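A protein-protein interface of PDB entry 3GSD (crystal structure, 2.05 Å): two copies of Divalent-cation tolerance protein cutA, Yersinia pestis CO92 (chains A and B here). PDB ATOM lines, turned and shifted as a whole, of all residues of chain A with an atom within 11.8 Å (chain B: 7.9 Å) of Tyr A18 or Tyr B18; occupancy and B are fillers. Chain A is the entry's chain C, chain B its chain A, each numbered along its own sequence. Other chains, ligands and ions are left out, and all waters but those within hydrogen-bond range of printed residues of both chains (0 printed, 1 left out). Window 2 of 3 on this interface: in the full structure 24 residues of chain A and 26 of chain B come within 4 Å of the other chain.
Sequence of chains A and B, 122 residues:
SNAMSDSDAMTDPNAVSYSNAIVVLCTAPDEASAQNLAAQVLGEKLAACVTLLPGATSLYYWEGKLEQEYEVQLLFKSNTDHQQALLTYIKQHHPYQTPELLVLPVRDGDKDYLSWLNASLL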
ATOM      1  N   TYR A  18       1.895   2.976   3.291  1.00  0.00           N
ATOM      2  CA  TYR A  18       2.452   3.966   4.266  1.00  0.00           C
ATOM      3  C   TYR A  18       3.972   3.997   4.262  1.00  0.00           C
ATOM      4  O   TYR A  18       4.628   2.946   4.330  1.00  0.00           O
ATOM      5  CB  TYR A  18       1.938   3.683   5.681  1.00  0.00           C
ATOM      6  CG  TYR A  18       0.555   4.234   5.969  1.00  0.00           C
ATOM      7  CD1 TYR A  18      -0.545   3.876   5.181  1.00  0.00           C
ATOM      8  CD2 TYR A  18       0.336   5.075   7.069  1.00  0.00           C
ATOM      9  CE1 TYR A  18      -1.825   4.378   5.453  1.00  0.00           C
ATOM     10  CE2 TYR A  18      -0.938   5.572   7.359  1.00  0.00           C
ATOM     11  CZ  TYR A  18      -2.015   5.221   6.546  1.00  0.00           C
ATOM     12  OH  TYR A  18      -3.276   5.706   6.826  1.00  0.00           O
ATOM     13  N   SER A  19       4.536   5.205   4.194  1.00  0.00           N
ATOM     14  CA  SER A  19       5.987   5.355   4.199  1.00  0.00           C
ATOM     15  C   SER A  19       6.480   5.093   5.613  1.00  0.00           C
ATOM     16  O   SER A  19       5.678   4.900   6.543  1.00  0.00           O
ATOM     17  CB  SER A  19       6.407   6.768   3.756  1.00  0.00           C
ATOM     18  OG  SER A  19       6.288   7.693   4.828  1.00  0.00           O
ATOM     19  N   ASN A  20       7.793   5.079   5.797  1.00  0.00           N
ATOM     20  CA  ASN A  20       8.328   4.854   7.116  1.00  0.00           C
ATOM     21  C   ASN A  20       8.586   6.170   7.870  1.00  0.00           C
ATOM     22  O   ASN A  20       9.074   6.155   8.987  1.00  0.00           O
ATOM     23  CB  ASN A  20       9.566   3.945   7.079  1.00  0.00           C
ATOM     24  CG  ASN A  20      10.730   4.565   6.353  1.00  0.00           C
ATOM     25  OD1 ASN A  20      10.580   5.543   5.627  1.00  0.00           O
ATOM     26  ND2 ASN A  20      11.914   3.982   6.536  1.00  0.00           N
ATOM     27  N   ALA A  21       8.237   7.303   7.253  1.00  0.00           N
ATOM     28  CA  ALA A  21       8.391   8.616   7.925  1.00  0.00           C
ATOM     29  C   ALA A  21       7.356   8.825   9.028  1.00  0.00           C
ATOM     30  O   ALA A  21       6.258   8.252   8.994  1.00  0.00           O
ATOM     31  CB  ALA A  21       8.334   9.765   6.928  1.00  0.00           C
ATOM     32  N   ILE A  22       7.710   9.652  10.005  1.00  0.00           N
ATOM     33  CA  ILE A  22       6.801   9.991  11.100  1.00  0.00           C
ATOM     34  C   ILE A  22       6.987  11.449  11.453  1.00  0.00           C
ATOM     35  O   ILE A  22       8.037  12.028  11.176  1.00  0.00           O
ATOM     36  CB  ILE A  22       7.072   9.156  12.402  1.00  0.00           C
ATOM     37  CG1 ILE A  22       8.527   9.347  12.880  1.00  0.00           C
ATOM     38  CG2 ILE A  22       6.688   7.654  12.205  1.00  0.00           C
ATOM     39  CD1 ILE A  22       8.840   8.759  14.289  1.00  0.00           C
ATOM     40  N   VAL A  23       5.961  12.048  12.051  1.00  0.00           N
ATOM     41  CA  VAL A  23       6.067  13.399  12.542  1.00  0.00           C
ATOM     42  C   VAL A  23       5.658  13.353  14.010  1.00  0.00           C
ATOM     43  O   VAL A  23       4.514  13.004  14.345  1.00  0.00           O
ATOM     44  CB  VAL A  23       5.186  14.401  11.784  1.00  0.00           C
ATOM     45  CG1 VAL A  23       5.305  15.782  12.444  1.00  0.00           C
ATOM     46  CG2 VAL A  23       5.591  14.474  10.318  1.00  0.00           C
ATOM     47  N   SER A  78      11.063  12.416  11.386  1.00  0.00           N
ATOM     48  CA  SER A  78      11.985  11.269  11.524  1.00  0.00           C
ATOM     49  C   SER A  78      11.382  10.026  10.854  1.00  0.00           C
ATOM     50  O   SER A  78      10.526  10.144   9.981  1.00  0.00           O
ATOM     51  CB  SER A  78      12.230  11.007  13.033  1.00  0.00           C
ATOM     52  OG  SER A  78      13.240  10.004  13.273  1.00  0.00           O
ATOM     53  N   ASN A  79      11.849   8.836  11.231  1.00  0.00           N
ATOM     54  CA  ASN A  79      11.260   7.610  10.686  1.00  0.00           C
ATOM     55  C   ASN A  79      11.000   6.562  11.763  1.00  0.00           C
ATOM     56  O   ASN A  79      11.493   6.682  12.897  1.00  0.00           O
ATOM     57  CB  ASN A  79      12.046   7.056   9.467  1.00  0.00           C
ATOM     58  CG  ASN A  79      13.424   6.536   9.823  1.00  0.00           C
ATOM     59  OD1 ASN A  79      13.717   6.227  10.981  1.00  0.00           O
ATOM     60  ND2 ASN A  79      14.278   6.408   8.810  1.00  0.00           N
ATOM     61  N   THR A  80      10.205   5.554  11.415  1.00  0.00           N
ATOM     62  CA  THR A  80       9.801   4.518  12.363  1.00  0.00           C
ATOM     63  C   THR A  80      10.982   3.782  12.979  1.00  0.00           C
ATOM     64  O   THR A  80      10.911   3.344  14.135  1.00  0.00           O
ATOM     65  CB  THR A  80       8.838   3.495  11.704  1.00  0.00           C
ATOM     66  OG1 THR A  80       9.495   2.877  10.588  1.00  0.00           O
ATOM     67  CG2 THR A  80       7.572   4.196  11.219  1.00  0.00           C
ATOM     68  N   ASP A  81      12.061   3.639  12.207  1.00  0.00           N
ATOM     69  CA  ASP A  81      13.264   2.963  12.690  1.00  0.00           C
ATOM     70  C   ASP A  81      13.923   3.690  13.849  1.00  0.00           C
ATOM     71  O   ASP A  81      14.652   3.080  14.620  1.00  0.00           O
ATOM     72  CB  ASP A  81      14.300   2.792  11.569  1.00  0.00           C
ATOM     73  CG  ASP A  81      14.001   1.607  10.661  1.00  0.00           C
ATOM     74  OD1 ASP A  81      13.004   0.879  10.890  1.00  0.00           O
ATOM     75  OD2 ASP A  81      14.783   1.392   9.712  1.00  0.00           O
ATOM     76  N   GLN A  83      12.053   5.852  15.800  1.00  0.00           N
ATOM     77  CA  GLN A  83      10.942   6.295  16.619  1.00  0.00           C
ATOM     78  C   GLN A  83      11.121   6.090  18.131  1.00  0.00           C
ATOM     79  O   GLN A  83      10.969   7.040  18.906  1.00  0.00           O
ATOM     80  CB  GLN A  83       9.650   5.656  16.121  1.00  0.00           C
ATOM     81  CG  GLN A  83       8.413   6.035  16.911  1.00  0.00           C
ATOM     82  CD  GLN A  83       7.179   5.329  16.383  1.00  0.00           C
ATOM     83  OE1 GLN A  83       6.887   5.364  15.179  1.00  0.00           O
ATOM     84  NE2 GLN A  83       6.446   4.691  17.275  1.00  0.00           N
ATOM     85  N   VAL A 103       3.123  10.470  18.071  1.00  0.00           N
ATOM     86  CA  VAL A 103       3.694  10.114  16.780  1.00  0.00           C
ATOM     87  C   VAL A 103       2.603  10.041  15.720  1.00  0.00           C
ATOM     88  O   VAL A 103       1.678   9.215  15.820  1.00  0.00           O
ATOM     89  CB  VAL A 103       4.422   8.752  16.842  1.00  0.00           C
ATOM     90  CG1 VAL A 103       5.131   8.461  15.506  1.00  0.00           C
ATOM     91  CG2 VAL A 103       5.434   8.727  18.014  1.00  0.00           C
ATOM     92  N   LEU A 104       2.701  10.922  14.718  1.00  0.00           N
ATOM     93  CA  LEU A 104       1.775  10.912  13.595  1.00  0.00           C
ATOM     94  C   LEU A 104       2.388  10.064  12.500  1.00  0.00           C
ATOM     95  O   LEU A 104       3.575  10.207  12.212  1.00  0.00           O
ATOM     96  CB  LEU A 104       1.539  12.334  13.047  1.00  0.00           C
ATOM     97  CG  LEU A 104       1.000  13.391  14.012  1.00  0.00           C
ATOM     98  CD1 LEU A 104       0.899  14.766  13.332  1.00  0.00           C
ATOM     99  CD2 LEU A 104      -0.334  12.957  14.568  1.00  0.00           C
ATOM    100  N   PRO A 105       1.583   9.169  11.877  1.00  0.00           N
ATOM    101  CA  PRO A 105       2.160   8.402  10.780  1.00  0.00           C
ATOM    102  C   PRO A 105       2.173   9.239   9.494  1.00  0.00           C
ATOM    103  O   PRO A 105       1.420  10.213   9.364  1.00  0.00           O
ATOM    104  CB  PRO A 105       1.196   7.202  10.638  1.00  0.00           C
ATOM    105  CG  PRO A 105      -0.141   7.759  11.062  1.00  0.00           C
ATOM    106  CD  PRO A 105       0.193   8.769  12.174  1.00  0.00           C
ATOM    107  N   VAL A 106       3.061   8.893   8.577  1.00  0.00           N
ATOM    108  CA  VAL A 106       3.129   9.576   7.305  1.00  0.00           C
ATOM    109  C   VAL A 106       2.757   8.539   6.251  1.00  0.00           C
ATOM    110  O   VAL A 106       3.420   7.514   6.117  1.00  0.00           O
ATOM    111  CB  VAL A 106       4.535  10.160   7.040  1.00  0.00           C
ATOM    112  CG1 VAL A 106       4.635  10.695   5.621  1.00  0.00           C
ATOM    113  CG2 VAL A 106       4.889  11.262   8.085  1.00  0.00           C
ATOM    114  N   ARG A 107       1.682   8.789   5.511  1.00  0.00           N
ATOM    115  CA  ARG A 107       1.244   7.843   4.485  1.00  0.00           C
ATOM    116  C   ARG A 107       2.184   7.824   3.287  1.00  0.00           C
ATOM    117  O   ARG A 107       2.446   6.764   2.719  1.00  0.00           O
ATOM    118  CB  ARG A 107      -0.169   8.176   3.997  1.00  0.00           C
ATOM    119  CG  ARG A 107      -0.659   7.281   2.865  1.00  0.00           C
ATOM    120  CD  ARG A 107      -1.725   8.004   2.026  1.00  0.00           C
ATOM    121  NE  ARG A 107      -2.935   8.300   2.782  1.00  0.00           N
ATOM    122  CZ  ARG A 107      -4.087   7.661   2.621  1.00  0.00           C
ATOM    123  NH1 ARG A 107      -4.195   6.716   1.703  1.00  0.00           N
ATOM    124  NH2 ARG A 107      -5.137   7.987   3.356  1.00  0.00           N
ATOM    125  N   ASP A 108       2.695   8.993   2.899  1.00  0.00           N
ATOM    126  CA  ASP A 108       3.537   9.065   1.709  1.00  0.00           C
ATOM    127  C   ASP A 108       4.313  10.375   1.715  1.00  0.00           C
ATOM    128  O   ASP A 108       4.098  11.222   2.581  1.00  0.00           O
ATOM    129  CB  ASP A 108       2.629   9.011   0.468  1.00  0.00           C
ATOM    130  CG  ASP A 108       3.367   8.608  -0.796  1.00  0.00           C
ATOM    131  OD1 ASP A 108       4.620   8.588  -0.813  1.00  0.00           O
ATOM    132  OD2 ASP A 108       2.676   8.310  -1.787  1.00  0.00           O
ATOM    133  N   GLY A 109       5.229  10.526   0.764  1.00  0.00           N
ATOM    134  CA  GLY A 109       6.017  11.746   0.641  1.00  0.00           C
ATOM    135  C   GLY A 109       6.791  11.787  -0.663  1.00  0.00           C
ATOM    136  O   GLY A 109       6.777  10.820  -1.441  1.00  0.00           O
ATOM    137  N   ASP A 110       7.441  12.918  -0.923  1.00  0.00           N
ATOM    138  CA  ASP A 110       8.262  13.052  -2.105  1.00  0.00           C
ATOM    139  C   ASP A 110       9.474  12.162  -1.866  1.00  0.00           C
ATOM    140  O   ASP A 110      10.098  12.248  -0.809  1.00  0.00           O
ATOM    141  CB  ASP A 110       8.732  14.480  -2.272  1.00  0.00           C
ATOM    142  CG  ASP A 110       9.702  14.633  -3.420  1.00  0.00           C
ATOM    143  OD1 ASP A 110       9.233  14.761  -4.567  1.00  0.00           O
ATOM    144  OD2 ASP A 110      10.934  14.651  -3.172  1.00  0.00           O
ATOM    145  N   LYS A 111       9.816  11.335  -2.851  1.00  0.00           N
ATOM    146  CA  LYS A 111      10.926  10.380  -2.717  1.00  0.00           C
ATOM    147  C   LYS A 111      12.290  11.023  -2.438  1.00  0.00           C
ATOM    148  O   LYS A 111      13.074  10.493  -1.642  1.00  0.00           O
ATOM    149  CB  LYS A 111      11.003   9.449  -3.933  1.00  0.00           C
ATOM    150  CG  LYS A 111      11.455  10.139  -5.199  1.00  0.00           C
ATOM    151  CD  LYS A 111      11.632   9.150  -6.361  1.00  0.00           C
ATOM    152  CE  LYS A 111      12.471   9.779  -7.484  1.00  0.00           C
ATOM    153  NZ  LYS A 111      11.917  11.085  -7.953  1.00  0.00           N
ATOM    154  N   LEU A 114      12.146  12.103   1.203  1.00  0.00           N
ATOM    155  CA  LEU A 114      12.213  10.927   2.069  1.00  0.00           C
ATOM    156  C   LEU A 114      13.610  10.334   2.084  1.00  0.00           C
ATOM    157  O   LEU A 114      14.095   9.880   3.130  1.00  0.00           O
ATOM    158  CB  LEU A 114      11.166   9.882   1.665  1.00  0.00           C
ATOM    159  CG  LEU A 114       9.733  10.313   2.004  1.00  0.00           C
ATOM    160  CD1 LEU A 114       8.695   9.368   1.399  1.00  0.00           C
ATOM    161  CD2 LEU A 114       9.567  10.411   3.528  1.00  0.00           C
ATOM    162  N   ASN A 118      15.760   9.872   5.453  1.00  0.00           N
ATOM    163  CA  ASN A 118      16.298   8.580   5.879  1.00  0.00           C
ATOM    164  C   ASN A 118      17.827   8.588   6.015  1.00  0.00           C
ATOM    165  O   ASN A 118      18.370   8.069   6.986  1.00  0.00           O
ATOM    166  CB  ASN A 118      15.825   7.454   4.949  1.00  0.00           C
ATOM    167  CG  ASN A 118      14.337   7.151   5.107  1.00  0.00           C
ATOM    168  OD1 ASN A 118      13.812   7.085   6.230  1.00  0.00           O
ATOM    169  ND2 ASN A 118      13.654   6.947   3.986  1.00  0.00           N
ATOM    170  N   TYR B  18     -10.953   4.835   7.328  1.00  0.00           N
ATOM    171  CA  TYR B  18     -10.256   6.127   7.004  1.00  0.00           C
ATOM    172  C   TYR B  18     -10.944   6.949   5.922  1.00  0.00           C
ATOM    173  O   TYR B  18     -11.543   6.400   4.983  1.00  0.00           O
ATOM    174  CB  TYR B  18      -8.792   5.873   6.631  1.00  0.00           C
ATOM    175  CG  TYR B  18      -7.886   5.720   7.837  1.00  0.00           C
ATOM    176  CD1 TYR B  18      -8.251   4.901   8.912  1.00  0.00           C
ATOM    177  CD2 TYR B  18      -6.648   6.364   7.889  1.00  0.00           C
ATOM    178  CE1 TYR B  18      -7.431   4.759  10.022  1.00  0.00           C
ATOM    179  CE2 TYR B  18      -5.809   6.215   8.991  1.00  0.00           C
ATOM    180  CZ  TYR B  18      -6.208   5.408  10.054  1.00  0.00           C
ATOM    181  OH  TYR B  18      -5.387   5.251  11.151  1.00  0.00           O
ATOM    182  N   SER B  19     -10.876   8.272   6.061  1.00  0.00           N
ATOM    183  CA  SER B  19     -11.452   9.140   5.061  1.00  0.00           C
ATOM    184  C   SER B  19     -10.431   9.241   3.936  1.00  0.00           C
ATOM    185  O   SER B  19      -9.328   8.700   4.034  1.00  0.00           O
ATOM    186  CB  SER B  19     -11.769  10.528   5.630  1.00  0.00           C
ATOM    187  OG  SER B  19     -10.593  11.296   5.812  1.00  0.00           O
ATOM    188  N   ASN B  20     -10.793   9.937   2.874  1.00  0.00           N
ATOM    189  CA  ASN B  20      -9.896  10.103   1.771  1.00  0.00           C
ATOM    190  C   ASN B  20      -9.167  11.446   1.853  1.00  0.00           C
ATOM    191  O   ASN B  20      -8.378  11.771   0.974  1.00  0.00           O
ATOM    192  CB  ASN B  20     -10.647   9.986   0.445  1.00  0.00           C
ATOM    193  CG  ASN B  20     -11.693  11.052   0.283  1.00  0.00           C
ATOM    194  OD1 ASN B  20     -12.191  11.605   1.268  1.00  0.00           O
ATOM    195  ND2 ASN B  20     -12.050  11.343  -0.956  1.00  0.00           N
ATOM    196  N   ALA B  21      -9.451  12.237   2.883  1.00  0.00           N
ATOM    197  CA  ALA B  21      -8.759  13.527   3.033  1.00  0.00           C
ATOM    198  C   ALA B  21      -7.315  13.311   3.474  1.00  0.00           C
ATOM    199  O   ALA B  21      -6.982  12.282   4.049  1.00  0.00           O
ATOM    200  CB  ALA B  21      -9.496  14.449   4.008  1.00  0.00           C
ATOM    201  N   VAL B 103       2.804  13.501   3.573  1.00  0.00           N
ATOM    202  CA  VAL B 103       1.365  13.345   3.556  1.00  0.00           C
ATOM    203  C   VAL B 103       0.877  12.671   4.817  1.00  0.00           C
ATOM    204  O   VAL B 103       1.255  11.524   5.100  1.00  0.00           O
ATOM    205  CB  VAL B 103       0.919  12.478   2.364  1.00  0.00           C
ATOM    206  CG1 VAL B 103      -0.609  12.394   2.328  1.00  0.00           C
ATOM    207  CG2 VAL B 103       1.471  13.041   1.065  1.00  0.00           C
ATOM    208  N   LEU B 104       0.049  13.379   5.580  1.00  0.00           N
ATOM    209  CA  LEU B 104      -0.556  12.826   6.783  1.00  0.00           C
ATOM    210  C   LEU B 104      -1.941  12.271   6.441  1.00  0.00           C
ATOM    211  O   LEU B 104      -2.725  12.937   5.752  1.00  0.00           O
ATOM    212  CB  LEU B 104      -0.705  13.903   7.858  1.00  0.00           C
ATOM    213  CG  LEU B 104       0.560  14.678   8.287  1.00  0.00           C
ATOM    214  CD1 LEU B 104       0.205  15.775   9.263  1.00  0.00           C
ATOM    215  CD2 LEU B 104       1.574  13.765   8.904  1.00  0.00           C
ATOM    216  N   PRO B 105      -2.237  11.031   6.896  1.00  0.00           N
ATOM    217  CA  PRO B 105      -3.576  10.496   6.645  1.00  0.00           C
ATOM    218  C   PRO B 105      -4.571  11.135   7.597  1.00  0.00           C
ATOM    219  O   PRO B 105      -4.185  11.640   8.638  1.00  0.00           O
ATOM    220  CB  PRO B 105      -3.430   8.998   6.975  1.00  0.00           C
ATOM    221  CG  PRO B 105      -2.337   8.958   8.035  1.00  0.00           C
ATOM    222  CD  PRO B 105      -1.370  10.074   7.633  1.00  0.00           C
ATOM    223  N   VAL B 106      -5.844  11.122   7.213  1.00  0.00           N
ATOM    224  CA  VAL B 106      -6.940  11.657   8.021  1.00  0.00           C
ATOM    225  C   VAL B 106      -7.868  10.476   8.293  1.00  0.00           C
ATOM    226  O   VAL B 106      -8.408   9.886   7.348  1.00  0.00           O
ATOM    227  CB  VAL B 106      -7.694  12.778   7.260  1.00  0.00           C
ATOM    228  CG1 VAL B 106      -8.977  13.189   8.010  1.00  0.00           C
ATOM    229  CG2 VAL B 106      -6.761  14.019   7.022  1.00  0.00           C
ATOM    230  N   ARG B 107      -8.058  10.117   9.562  1.00  0.00           N
ATOM    231  CA  ARG B 107      -8.872   8.937   9.873  1.00  0.00           C
ATOM    232  C   ARG B 107     -10.353   9.221   9.711  1.00  0.00           C
ATOM    233  O   ARG B 107     -11.120   8.334   9.343  1.00  0.00           O
ATOM    234  CB  ARG B 107      -8.569   8.381  11.282  1.00  0.00           C
ATOM    235  CG  ARG B 107      -9.387   8.977  12.414  1.00  0.00           C
ATOM    236  CD  ARG B 107      -8.938   8.468  13.803  1.00  0.00           C
ATOM    237  NE  ARG B 107      -9.008   7.015  13.953  1.00  0.00           N
ATOM    238  CZ  ARG B 107     -10.007   6.343  14.528  1.00  0.00           C
ATOM    239  NH1 ARG B 107     -11.060   6.968  15.021  1.00  0.00           N
ATOM    240  NH2 ARG B 107      -9.948   5.029  14.607  1.00  0.00           N
ATOM    241  N   ASP B 108     -10.760  10.461   9.995  1.00  0.00           N
ATOM    242  CA  ASP B 108     -12.165  10.845   9.873  1.00  0.00           C
ATOM    243  C   ASP B 108     -12.286  12.355   9.822  1.00  0.00           C
ATOM    244  O   ASP B 108     -11.329  13.072  10.096  1.00  0.00           O
ATOM    245  CB  ASP B 108     -12.956  10.314  11.067  1.00  0.00           C
ATOM    246  CG  ASP B 108     -14.394   9.940  10.702  1.00  0.00           C
ATOM    247  OD1 ASP B 108     -14.840   8.883  11.183  1.00  0.00           O
ATOM    248  OD2 ASP B 108     -15.054  10.656   9.890  1.00  0.00           O
ATOM    249  N   GLY B 109     -13.475  12.837   9.486  1.00  0.00           N
ATOM    250  CA  GLY B 109     -13.731  14.269   9.442  1.00  0.00           C
ATOM    251  C   GLY B 109     -15.214  14.577   9.468  1.00  0.00           C
ATOM    252  O   GLY B 109     -16.053  13.677   9.329  1.00  0.00           O
ATOM    253  N   LEU B 114     -15.785  17.701   4.784  1.00  0.00           N
ATOM    254  CA  LEU B 114     -15.215  16.798   3.769  1.00  0.00           C
ATOM    255  C   LEU B 114     -15.924  16.981   2.418  1.00  0.00           C
ATOM    256  O   LEU B 114     -15.283  16.948   1.362  1.00  0.00           O
ATOM    257  CB  LEU B 114     -15.263  15.334   4.226  1.00  0.00           C
ATOM    258  CG  LEU B 114     -14.361  14.958   5.418  1.00  0.00           C
ATOM    259  CD1 LEU B 114     -14.539  13.491   5.789  1.00  0.00           C
ATOM    260  CD2 LEU B 114     -12.906  15.249   5.094  1.00  0.00           C
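The side-chain hydroxyl (OG) of Ser A19 lies within hydrogen-bond range of the backbone carbonyl oxygen (O) of Val A106.
O of Arg A107 lies within hydrogen-bond range of N of Ser A19 (3.0 Å).
O of Ala A21 sits close to N of Val A106.
Among the printed residues, pairs that only touch across the chains: Pro A105 with Pro B105, Tyr A18 with Pro B105, Tyr A18 with Tyr B18, Val A106 with Val B103, Pro A105 with Leu B104 and Arg A107 with Pro B105.
Pro A105 touches Leu B104, but with the chains exchanged Leu A104 does not touch Pro B105 (6.1 Å).
Pro A105 touches its own counterpart, Pro B105.
Arg A107 touches Val B103, but with the chains exchanged Val A103 does not touch Arg B107 (10.8 Å).
Arg A107 touches Pro B105, but with the chains exchanged Pro A105 does not touch Arg B107 (8.4 Å).
12 positions are printed for both chains.
Of the 8 pairs that touch across the chains among the printed residues, 2 have their exchanged pair printed and touching as well.
The backbone NH (N) of Val B103 sits at hydrogen-bond distance from the backbone carbonyl oxygen (O) of Asp A108.
N of Arg A107 is in hydrogen-bond range of O of Val B103, at 2.8 Å.
Of the 12 printed residues of chain B, 4 touch a printed residue of chain A.
Hydrophobic or aromatic side chains of chain B that line the printed part of chain A: Tyr B18, Val B103, Leu B104 and Pro B105.
Of the 22 printed residues of chain A, 5 touch a printed residue of chain B.
Hydrophobic or aromatic side chains of chain A that line the printed part of chain B: Tyr A18, Pro A105 and Val A106.
Along chain A the printed residues that touch a printed residue of chain B span positions 18 to 108.
Among the printed residues, 8 pairs touch across the chains.
Of chain B, only Tyr B18 (3.4 Å) and Pro B105 (3.3 Å) come within 4 Å of Tyr A18.
Printed residues of chain A within 4 Å of Tyr B18: Tyr A18 (3.4 Å).
No residue of chain A comes within 4 Å of Ser B19.
No residue of chain A comes within 4 Å of Asn B20.
No residue of chain A comes within 4 Å of Val B106.
No residue of chain A comes within 4 Å of Arg B107.
No residue of chain A comes within 4 Å of Asp B108.
Of the printed residues of chain A, Pro B105 touches Tyr A18, Pro A105 and Arg A107.
Printed residues of chain B within 4 Å of Asp A108: Val B103.
Of the printed residues of chain A, Val B103 touches Val A106 (3.5 Å), Arg A107 (2.8 Å) and Asp A108 (2.8 Å).
Gln A83 touches none of the printed residues of chain B.
The nearest printed residue of chain A that does not touch Tyr B18 is Arg A107 (5.0 Å).
The nearest printed residue of chain B that does not touch Val A106 is Leu B104 (4.2 Å).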
